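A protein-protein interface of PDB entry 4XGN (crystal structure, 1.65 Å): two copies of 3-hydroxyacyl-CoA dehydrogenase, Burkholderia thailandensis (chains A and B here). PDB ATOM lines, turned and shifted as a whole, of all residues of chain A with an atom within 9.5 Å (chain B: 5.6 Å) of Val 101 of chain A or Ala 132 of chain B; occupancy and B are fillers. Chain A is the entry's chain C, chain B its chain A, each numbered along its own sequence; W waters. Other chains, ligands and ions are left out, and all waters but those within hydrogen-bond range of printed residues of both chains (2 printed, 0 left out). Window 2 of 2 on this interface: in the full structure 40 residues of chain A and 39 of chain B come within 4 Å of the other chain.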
ATOM      1  N   ALA A  98      -3.710 -15.830 -12.317  1.00  0.00           N
ATOM      2  CA  ALA A  98      -2.687 -16.556 -13.080  1.00  0.00           C
ATOM      3  C   ALA A  98      -3.057 -16.498 -14.551  1.00  0.00           C
ATOM      4  O   ALA A  98      -4.196 -16.746 -14.901  1.00  0.00           O
ATOM      5  CB  ALA A  98      -2.630 -17.978 -12.613  1.00  0.00           C
ATOM      6  N   LYS A  99      -2.070 -16.213 -15.405  1.00  0.00           N
ATOM      7  CA  LYS A  99      -2.287 -16.210 -16.826  1.00  0.00           C
ATOM      8  C   LYS A  99      -2.392 -17.619 -17.409  1.00  0.00           C
ATOM      9  O   LYS A  99      -1.771 -18.568 -16.932  1.00  0.00           O
ATOM     10  CB  LYS A  99      -1.191 -15.438 -17.550  1.00  0.00           C
ATOM     11  CG  LYS A  99      -1.075 -13.983 -17.099  1.00  0.00           C
ATOM     12  CD  LYS A  99      -0.023 -13.235 -17.928  1.00  0.00           C
ATOM     13  CE  LYS A  99       0.772 -12.227 -17.100  1.00  0.00           C
ATOM     14  NZ  LYS A  99       1.275 -11.058 -17.910  1.00  0.00           N
ATOM     15  N   THR A 100      -3.152 -17.729 -18.486  1.00  0.00           N
ATOM     16  CA  THR A 100      -3.259 -18.950 -19.245  1.00  0.00           C
ATOM     17  C   THR A 100      -1.891 -19.499 -19.595  1.00  0.00           C
ATOM     18  O   THR A 100      -1.655 -20.665 -19.376  1.00  0.00           O
ATOM     19  CB  THR A 100      -4.088 -18.740 -20.523  1.00  0.00           C
ATOM     20  OG1 THR A 100      -5.362 -18.286 -20.129  1.00  0.00           O
ATOM     21  CG2 THR A 100      -4.260 -20.029 -21.281  1.00  0.00           C
ATOM     22  N   VAL A 101      -1.007 -18.639 -20.086  1.00  0.00           N
ATOM     23  CA  VAL A 101       0.404 -18.999 -20.288  1.00  0.00           C
ATOM     24  C   VAL A 101       1.254 -17.986 -19.534  1.00  0.00           C
ATOM     25  O   VAL A 101       1.270 -16.804 -19.875  1.00  0.00           O
ATOM     26  CB  VAL A 101       0.829 -19.024 -21.764  1.00  0.00           C
ATOM     27  CG1 VAL A 101       2.306 -19.438 -21.837  1.00  0.00           C
ATOM     28  CG2 VAL A 101      -0.031 -20.020 -22.538  1.00  0.00           C
ATOM     29  N   GLY A 102       1.934 -18.457 -18.498  1.00  0.00           N
ATOM     30  CA  GLY A 102       2.773 -17.600 -17.675  1.00  0.00           C
ATOM     31  C   GLY A 102       4.216 -17.709 -18.110  1.00  0.00           C
ATOM     32  O   GLY A 102       4.545 -18.463 -19.033  1.00  0.00           O
ATOM     33  N   LYS A 103       5.086 -16.962 -17.425  1.00  0.00           N
ATOM     34  CA  LYS A 103       6.525 -17.027 -17.659  1.00  0.00           C
ATOM     35  C   LYS A 103       7.080 -18.454 -17.539  1.00  0.00           C
ATOM     36  O   LYS A 103       7.944 -18.848 -18.322  1.00  0.00           O
ATOM     37  CB  LYS A 103       7.280 -16.129 -16.660  1.00  0.00           C
ATOM     38  N   ASP A 104       6.548 -19.214 -16.583  1.00  0.00           N
ATOM     39  CA  ASP A 104       7.046 -20.552 -16.227  1.00  0.00           C
ATOM     40  C   ASP A 104       6.269 -21.724 -16.828  1.00  0.00           C
ATOM     41  O   ASP A 104       6.572 -22.878 -16.541  1.00  0.00           O
ATOM     42  CB  ASP A 104       7.057 -20.700 -14.697  1.00  0.00           C
ATOM     43  CG  ASP A 104       8.024 -19.735 -14.020  1.00  0.00           C
ATOM     44  OD1 ASP A 104       9.061 -19.395 -14.644  1.00  0.00           O
ATOM     45  OD2 ASP A 104       7.725 -19.321 -12.863  1.00  0.00           O
ATOM     46  N   GLY A 105       5.301 -21.450 -17.680  1.00  0.00           N
ATOM     47  CA  GLY A 105       4.549 -22.507 -18.312  1.00  0.00           C
ATOM     48  C   GLY A 105       3.076 -22.189 -18.201  1.00  0.00           C
ATOM     49  O   GLY A 105       2.694 -21.132 -17.715  1.00  0.00           O
ATOM     50  N   PRO A 106       2.236 -23.124 -18.599  1.00  0.00           N
ATOM     51  CA  PRO A 106       0.792 -22.908 -18.495  1.00  0.00           C
ATOM     52  C   PRO A 106       0.287 -22.721 -17.081  1.00  0.00           C
ATOM     53  O   PRO A 106       0.875 -23.248 -16.145  1.00  0.00           O
ATOM     54  CB  PRO A 106       0.201 -24.190 -19.063  1.00  0.00           C
ATOM     55  CG  PRO A 106       1.300 -25.168 -19.098  1.00  0.00           C
ATOM     56  CD  PRO A 106       2.568 -24.425 -19.195  1.00  0.00           C
ATOM     57  N   HIS A 107      -0.827 -21.988 -16.963  1.00  0.00           N
ATOM     58  CA  HIS A 107      -1.656 -21.905 -15.747  1.00  0.00           C
ATOM     59  C   HIS A 107      -1.741 -23.285 -15.099  1.00  0.00           C
ATOM     60  O   HIS A 107      -2.105 -24.236 -15.756  1.00  0.00           O
ATOM     61  CB  HIS A 107      -3.062 -21.480 -16.191  1.00  0.00           C
ATOM     62  CG  HIS A 107      -3.994 -21.054 -15.097  1.00  0.00           C
ATOM     63  ND1 HIS A 107      -4.352 -21.856 -14.038  1.00  0.00           N
ATOM     64  CD2 HIS A 107      -4.739 -19.928 -14.979  1.00  0.00           C
ATOM     65  CE1 HIS A 107      -5.245 -21.221 -13.289  1.00  0.00           C
ATOM     66  NE2 HIS A 107      -5.503 -20.055 -13.847  1.00  0.00           N
ATOM     67  N   PRO A 108      -1.406 -23.405 -13.804  1.00  0.00           N
ATOM     68  CA  PRO A 108      -1.545 -24.739 -13.207  1.00  0.00           C
ATOM     69  C   PRO A 108      -2.981 -25.210 -13.217  1.00  0.00           C
ATOM     70  O   PRO A 108      -3.906 -24.411 -12.934  1.00  0.00           O
ATOM     71  CB  PRO A 108      -1.060 -24.527 -11.761  1.00  0.00           C
ATOM     72  CG  PRO A 108      -0.111 -23.372 -11.851  1.00  0.00           C
ATOM     73  CD  PRO A 108      -0.676 -22.470 -12.920  1.00  0.00           C
ATOM     74  N   ILE A 161      -6.739  -9.900 -17.863  1.00  0.00           N
ATOM     75  CA  ILE A 161      -5.535 -10.737 -17.907  1.00  0.00           C
ATOM     76  C   ILE A 161      -5.278 -11.307 -16.500  1.00  0.00           C
ATOM     77  O   ILE A 161      -5.368 -10.599 -15.517  1.00  0.00           O
ATOM     78  CB  ILE A 161      -4.301  -9.945 -18.391  1.00  0.00           C
ATOM     79  CG1 ILE A 161      -4.473  -9.529 -19.849  1.00  0.00           C
ATOM     80  CG2 ILE A 161      -3.004 -10.731 -18.214  1.00  0.00           C
ATOM     81  CD1 ILE A 161      -3.473  -8.509 -20.383  1.00  0.00           C
ATOM     82  N   GLY A 162      -5.059 -12.613 -16.424  1.00  0.00           N
ATOM     83  CA  GLY A 162      -4.878 -13.262 -15.169  1.00  0.00           C
ATOM     84  C   GLY A 162      -6.124 -13.787 -14.476  1.00  0.00           C
ATOM     85  O   GLY A 162      -6.006 -14.516 -13.488  1.00  0.00           O
ATOM     86  N   ALA A 164      -8.735 -15.792 -15.952  1.00  0.00           N
ATOM     87  CA  ALA A 164      -9.497 -16.838 -16.646  1.00  0.00           C
ATOM     88  C   ALA A 164     -10.264 -17.748 -15.675  1.00  0.00           C
ATOM     89  O   ALA A 164     -11.435 -18.060 -15.919  1.00  0.00           O
ATOM     90  CB  ALA A 164      -8.617 -17.693 -17.534  1.00  0.00           C
ATOM     91  N   ILE B 127      -6.874 -25.874 -23.450  1.00  0.00           N
ATOM     92  CA  ILE B 127      -6.426 -24.541 -23.889  1.00  0.00           C
ATOM     93  C   ILE B 127      -5.040 -24.193 -23.355  1.00  0.00           C
ATOM     94  O   ILE B 127      -4.190 -23.745 -24.110  1.00  0.00           O
ATOM     95  CB  ILE B 127      -7.451 -23.447 -23.484  1.00  0.00           C
ATOM     96  CG1 ILE B 127      -8.765 -23.592 -24.301  1.00  0.00           C
ATOM     97  CG2 ILE B 127      -6.862 -22.036 -23.561  1.00  0.00           C
ATOM     98  CD1 ILE B 127      -9.888 -22.694 -23.835  1.00  0.00           C
ATOM     99  N   ARG B 128      -4.794 -24.422 -22.079  1.00  0.00           N
ATOM    100  CA  ARG B 128      -3.569 -23.937 -21.491  1.00  0.00           C
ATOM    101  C   ARG B 128      -2.367 -24.687 -22.082  1.00  0.00           C
ATOM    102  O   ARG B 128      -1.327 -24.079 -22.317  1.00  0.00           O
ATOM    103  CB  ARG B 128      -3.653 -24.054 -19.960  1.00  0.00           C
ATOM    104  CG  ARG B 128      -3.544 -25.469 -19.421  1.00  0.00           C
ATOM    105  CD  ARG B 128      -3.972 -25.656 -17.969  1.00  0.00           C
ATOM    106  NE  ARG B 128      -3.726 -27.069 -17.716  1.00  0.00           N
ATOM    107  CZ  ARG B 128      -2.553 -27.585 -17.328  1.00  0.00           C
ATOM    108  NH1 ARG B 128      -1.562 -26.825 -16.881  1.00  0.00           N
ATOM    109  NH2 ARG B 128      -2.390 -28.903 -17.354  1.00  0.00           N
ATOM    110  N   VAL B 129      -2.538 -25.984 -22.341  1.00  0.00           N
ATOM    111  CA  VAL B 129      -1.465 -26.795 -22.852  1.00  0.00           C
ATOM    112  C   VAL B 129      -1.225 -26.508 -24.343  1.00  0.00           C
ATOM    113  O   VAL B 129      -0.056 -26.326 -24.805  1.00  0.00           O
ATOM    114  CB  VAL B 129      -1.703 -28.300 -22.561  1.00  0.00           C
ATOM    115  CG1 VAL B 129      -0.557 -29.135 -23.125  1.00  0.00           C
ATOM    116  CG2 VAL B 129      -1.807 -28.562 -21.052  1.00  0.00           C
ATOM    117  N   ALA B 130      -2.316 -26.488 -25.116  1.00  0.00           N
ATOM    118  CA  ALA B 130      -2.222 -26.102 -26.519  1.00  0.00           C
ATOM    119  C   ALA B 130      -1.691 -24.675 -26.731  1.00  0.00           C
ATOM    120  O   ALA B 130      -0.889 -24.453 -27.635  1.00  0.00           O
ATOM    121  CB  ALA B 130      -3.549 -26.286 -27.225  1.00  0.00           C
ATOM    122  N   ALA B 131      -2.111 -23.726 -25.889  1.00  0.00           N
ATOM    123  CA  ALA B 131      -1.637 -22.359 -25.998  1.00  0.00           C
ATOM    124  C   ALA B 131      -0.135 -22.248 -25.729  1.00  0.00           C
ATOM    125  O   ALA B 131       0.567 -21.503 -26.407  1.00  0.00           O
ATOM    126  CB  ALA B 131      -2.425 -21.456 -25.044  1.00  0.00           C
ATOM    127  N   ALA B 132       0.340 -22.980 -24.737  1.00  0.00           N
ATOM    128  CA  ALA B 132       1.761 -22.956 -24.429  1.00  0.00           C
ATOM    129  C   ALA B 132       2.548 -23.460 -25.665  1.00  0.00           C
ATOM    130  O   ALA B 132       3.593 -22.904 -25.992  1.00  0.00           O
ATOM    131  CB  ALA B 132       2.059 -23.810 -23.237  1.00  0.00           C
ATOM    132  N   ALA B 133       2.024 -24.472 -26.350  1.00  0.00           N
ATOM    133  CA  ALA B 133       2.703 -25.009 -27.538  1.00  0.00           C
ATOM    134  C   ALA B 133       2.618 -24.048 -28.714  1.00  0.00           C
ATOM    135  O   ALA B 133       3.606 -23.854 -29.455  1.00  0.00           O
ATOM    136  CB  ALA B 133       2.141 -26.378 -27.907  1.00  0.00           C
ATOM    137  N   MET B 134       1.449 -23.444 -28.924  1.00  0.00           N
ATOM    138  CA  MET B 134       1.304 -22.464 -30.017  1.00  0.00           C
ATOM    139  C   MET B 134       2.157 -21.227 -29.803  1.00  0.00           C
ATOM    140  O   MET B 134       2.660 -20.674 -30.759  1.00  0.00           O
ATOM    141  CB  MET B 134      -0.131 -22.036 -30.202  1.00  0.00           C
ATOM    142  CG  MET B 134      -1.118 -23.090 -30.662  1.00  0.00           C
ATOM    143  SD  MET B 134      -2.802 -22.396 -30.357  1.00  0.00           S
ATOM    144  CE  MET B 134      -3.714 -23.677 -31.218  1.00  0.00           C
ATOM    145  N   ALA B 135       2.341 -20.805 -28.551  1.00  0.00           N
ATOM    146  CA  ALA B 135       3.135 -19.613 -28.227  1.00  0.00           C
ATOM    147  C   ALA B 135       4.598 -19.745 -28.725  1.00  0.00           C
ATOM    148  O   ALA B 135       5.273 -18.743 -28.945  1.00  0.00           O
ATOM    149  CB  ALA B 135       3.124 -19.383 -26.730  1.00  0.00           C
ATOM    150  N   ALA B 136       5.049 -20.981 -28.906  1.00  0.00           N
ATOM    151  CA  ALA B 136       6.370 -21.260 -29.412  1.00  0.00           C
ATOM    152  C   ALA B 136       6.460 -21.275 -30.930  1.00  0.00           C
ATOM    153  O   ALA B 136       7.581 -21.358 -31.482  1.00  0.00           O
ATOM    154  CB  ALA B 136       6.869 -22.578 -28.820  1.00  0.00           C
ATOM    155  N   ASP B 183      -5.213 -12.686 -22.279  1.00  0.00           N
ATOM    156  CA  ASP B 183      -4.002 -13.375 -21.831  1.00  0.00           C
ATOM    157  C   ASP B 183      -3.087 -13.710 -22.998  1.00  0.00           C
ATOM    158  O   ASP B 183      -1.868 -13.596 -22.867  1.00  0.00           O
ATOM    159  CB  ASP B 183      -4.341 -14.740 -21.193  1.00  0.00           C
ATOM    160  CG  ASP B 183      -4.698 -14.663 -19.755  1.00  0.00           C
ATOM    161  OD1 ASP B 183      -4.645 -13.566 -19.147  1.00  0.00           O
ATOM    162  OD2 ASP B 183      -5.121 -15.701 -19.232  1.00  0.00           O
ATOM    163  N   LEU B 184      -3.686 -14.147 -24.116  1.00  0.00           N
ATOM    164  CA  LEU B 184      -2.935 -14.675 -25.254  1.00  0.00           C
ATOM    165  C   LEU B 184      -2.688 -13.673 -26.354  1.00  0.00           C
ATOM    166  O   LEU B 184      -2.045 -14.019 -27.382  1.00  0.00           O
ATOM    167  CB  LEU B 184      -3.634 -15.921 -25.780  1.00  0.00           C
ATOM    168  CG  LEU B 184      -3.751 -17.062 -24.784  1.00  0.00           C
ATOM    169  CD1 LEU B 184      -4.445 -18.263 -25.377  1.00  0.00           C
ATOM    170  CD2 LEU B 184      -2.411 -17.462 -24.164  1.00  0.00           C
ATOM    171  N   ASN B 187       0.873 -13.293 -27.368  1.00  0.00           N
ATOM    172  CA  ASN B 187       1.307 -14.519 -28.066  1.00  0.00           C
ATOM    173  C   ASN B 187       0.735 -14.643 -29.449  1.00  0.00           C
ATOM    174  O   ASN B 187       1.121 -15.521 -30.176  1.00  0.00           O
ATOM    175  CB  ASN B 187       0.924 -15.770 -27.252  1.00  0.00           C
ATOM    176  CG  ASN B 187       1.425 -15.701 -25.831  1.00  0.00           C
ATOM    177  OD1 ASN B 187       0.660 -15.418 -24.906  1.00  0.00           O
ATOM    178  ND2 ASN B 187       2.719 -15.932 -25.643  1.00  0.00           N
HETATM  179  O   HOH W   1      -5.992 -15.755 -16.741  1.00  0.00           O
HETATM  180  O   HOH W   2      -1.072 -15.812 -20.985  1.00  0.00           O
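Water W1 lies within hydrogen-bond range of OD2 of Asp 183 of chain B (2.6 Å), O of Ala 98 of chain A (2.8 Å), N of Ala 164 of chain A (2.9 Å) and N of Gly 162 of chain A (3.3 Å).
Water W2 lies within hydrogen-bond range of the backbone carbonyl oxygen of Val 101 of chain A (2.8 Å) and the backbone carbonyl oxygen of Asp 183 of chain B (3.0 Å).
Lys 99 of chain A touches Asp 183 of chain B (CA to OD2, 3.8 Å).
CG2 of Thr 100 of chain A touches CG2 of Ile 127 of chain B, 3.9996 Å away.
CG2 of Thr 100 of chain A touches CA of Arg 128 of chain B (3.97 Å).
Ala 131 of chain B touches Val 101 of chain A.
Ala 132 of chain B touches Val 101 of chain A (N to CG2, 3.7 Å).
Leu 184 of chain B touches Val 101 of chain A (CD2 to CG2, 3.9 Å).
Arg 128 of chain B touches Pro 106 of chain A (O to CB, 3.6 Å).
Asp 183 of chain B touches Ile 161 of chain A.
No position is printed for both chains.
Of chain B, only Ala 131 (3.8 Å), Ala 132 (3.7 Å) and Leu 184 (3.9 Å) come within 4 Å of Val 101 of chain A.
Of chain A, only Val 101 (3.8 Å) comes within 4 Å of Ala 131 of chain B.
Of the printed residues of chain B, Thr 100 of chain A touches Ile 127, Arg 128 and Asp 183.
Of the printed residues of chain A, Asp 183 of chain B touches Lys 99, Thr 100, Ile 161 and Gly 162.
Of the printed residues of chain A, Arg 128 of chain B touches Thr 100, Pro 106 and His 107.
Of the printed residues of chain B, His 107 of chain A touches Arg 128.
Pro 108 of chain A touches none of the printed residues of chain B.
Val 129 of chain B touches none of the printed residues of chain A.
The nearest residue of chain B that does not touch Val 101 of chain A is Arg 128 of chain B (4.3 Å).
The nearest printed residue of chain B that does not touch Thr 100 of chain A is Leu 184 of chain B (4.2 Å).
The backbone NH (N) of Ala 98 of chain A lies within hydrogen-bond range of the backbone carbonyl oxygen (O) of Gly 162 of chain A.
The backbone NH of His 107 of chain A is in hydrogen-bond range of the backbone carbonyl oxygen of Thr 100 of chain A, 2.9 Å away.
Hydrophobic or aromatic side chains of chain B within 4 Å of the printed part of chain A: Ile 127, Ala 131 and Leu 184.
Among the printed residues, no Asp or Glu carboxylate lies within 4 Å of a Lys or Arg side-chain nitrogen of the other chain.
The backbone NH (N) of Gly 162 of chain A is in hydrogen-bond range of the side-chain carboxylate (OD1) of Asp 183 of chain B (2.9 Å).
The guanidinium group (NH1) of Arg 128 of chain B sits at hydrogen-bond distance from the backbone carbonyl oxygen (O) of His 107 of chain A.
The side-chain carboxylate (OD2) of Asp 183 of chain B sits at hydrogen-bond distance from the side-chain hydroxyl (OG1) of Thr 100 of chain A (2.7 Å).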
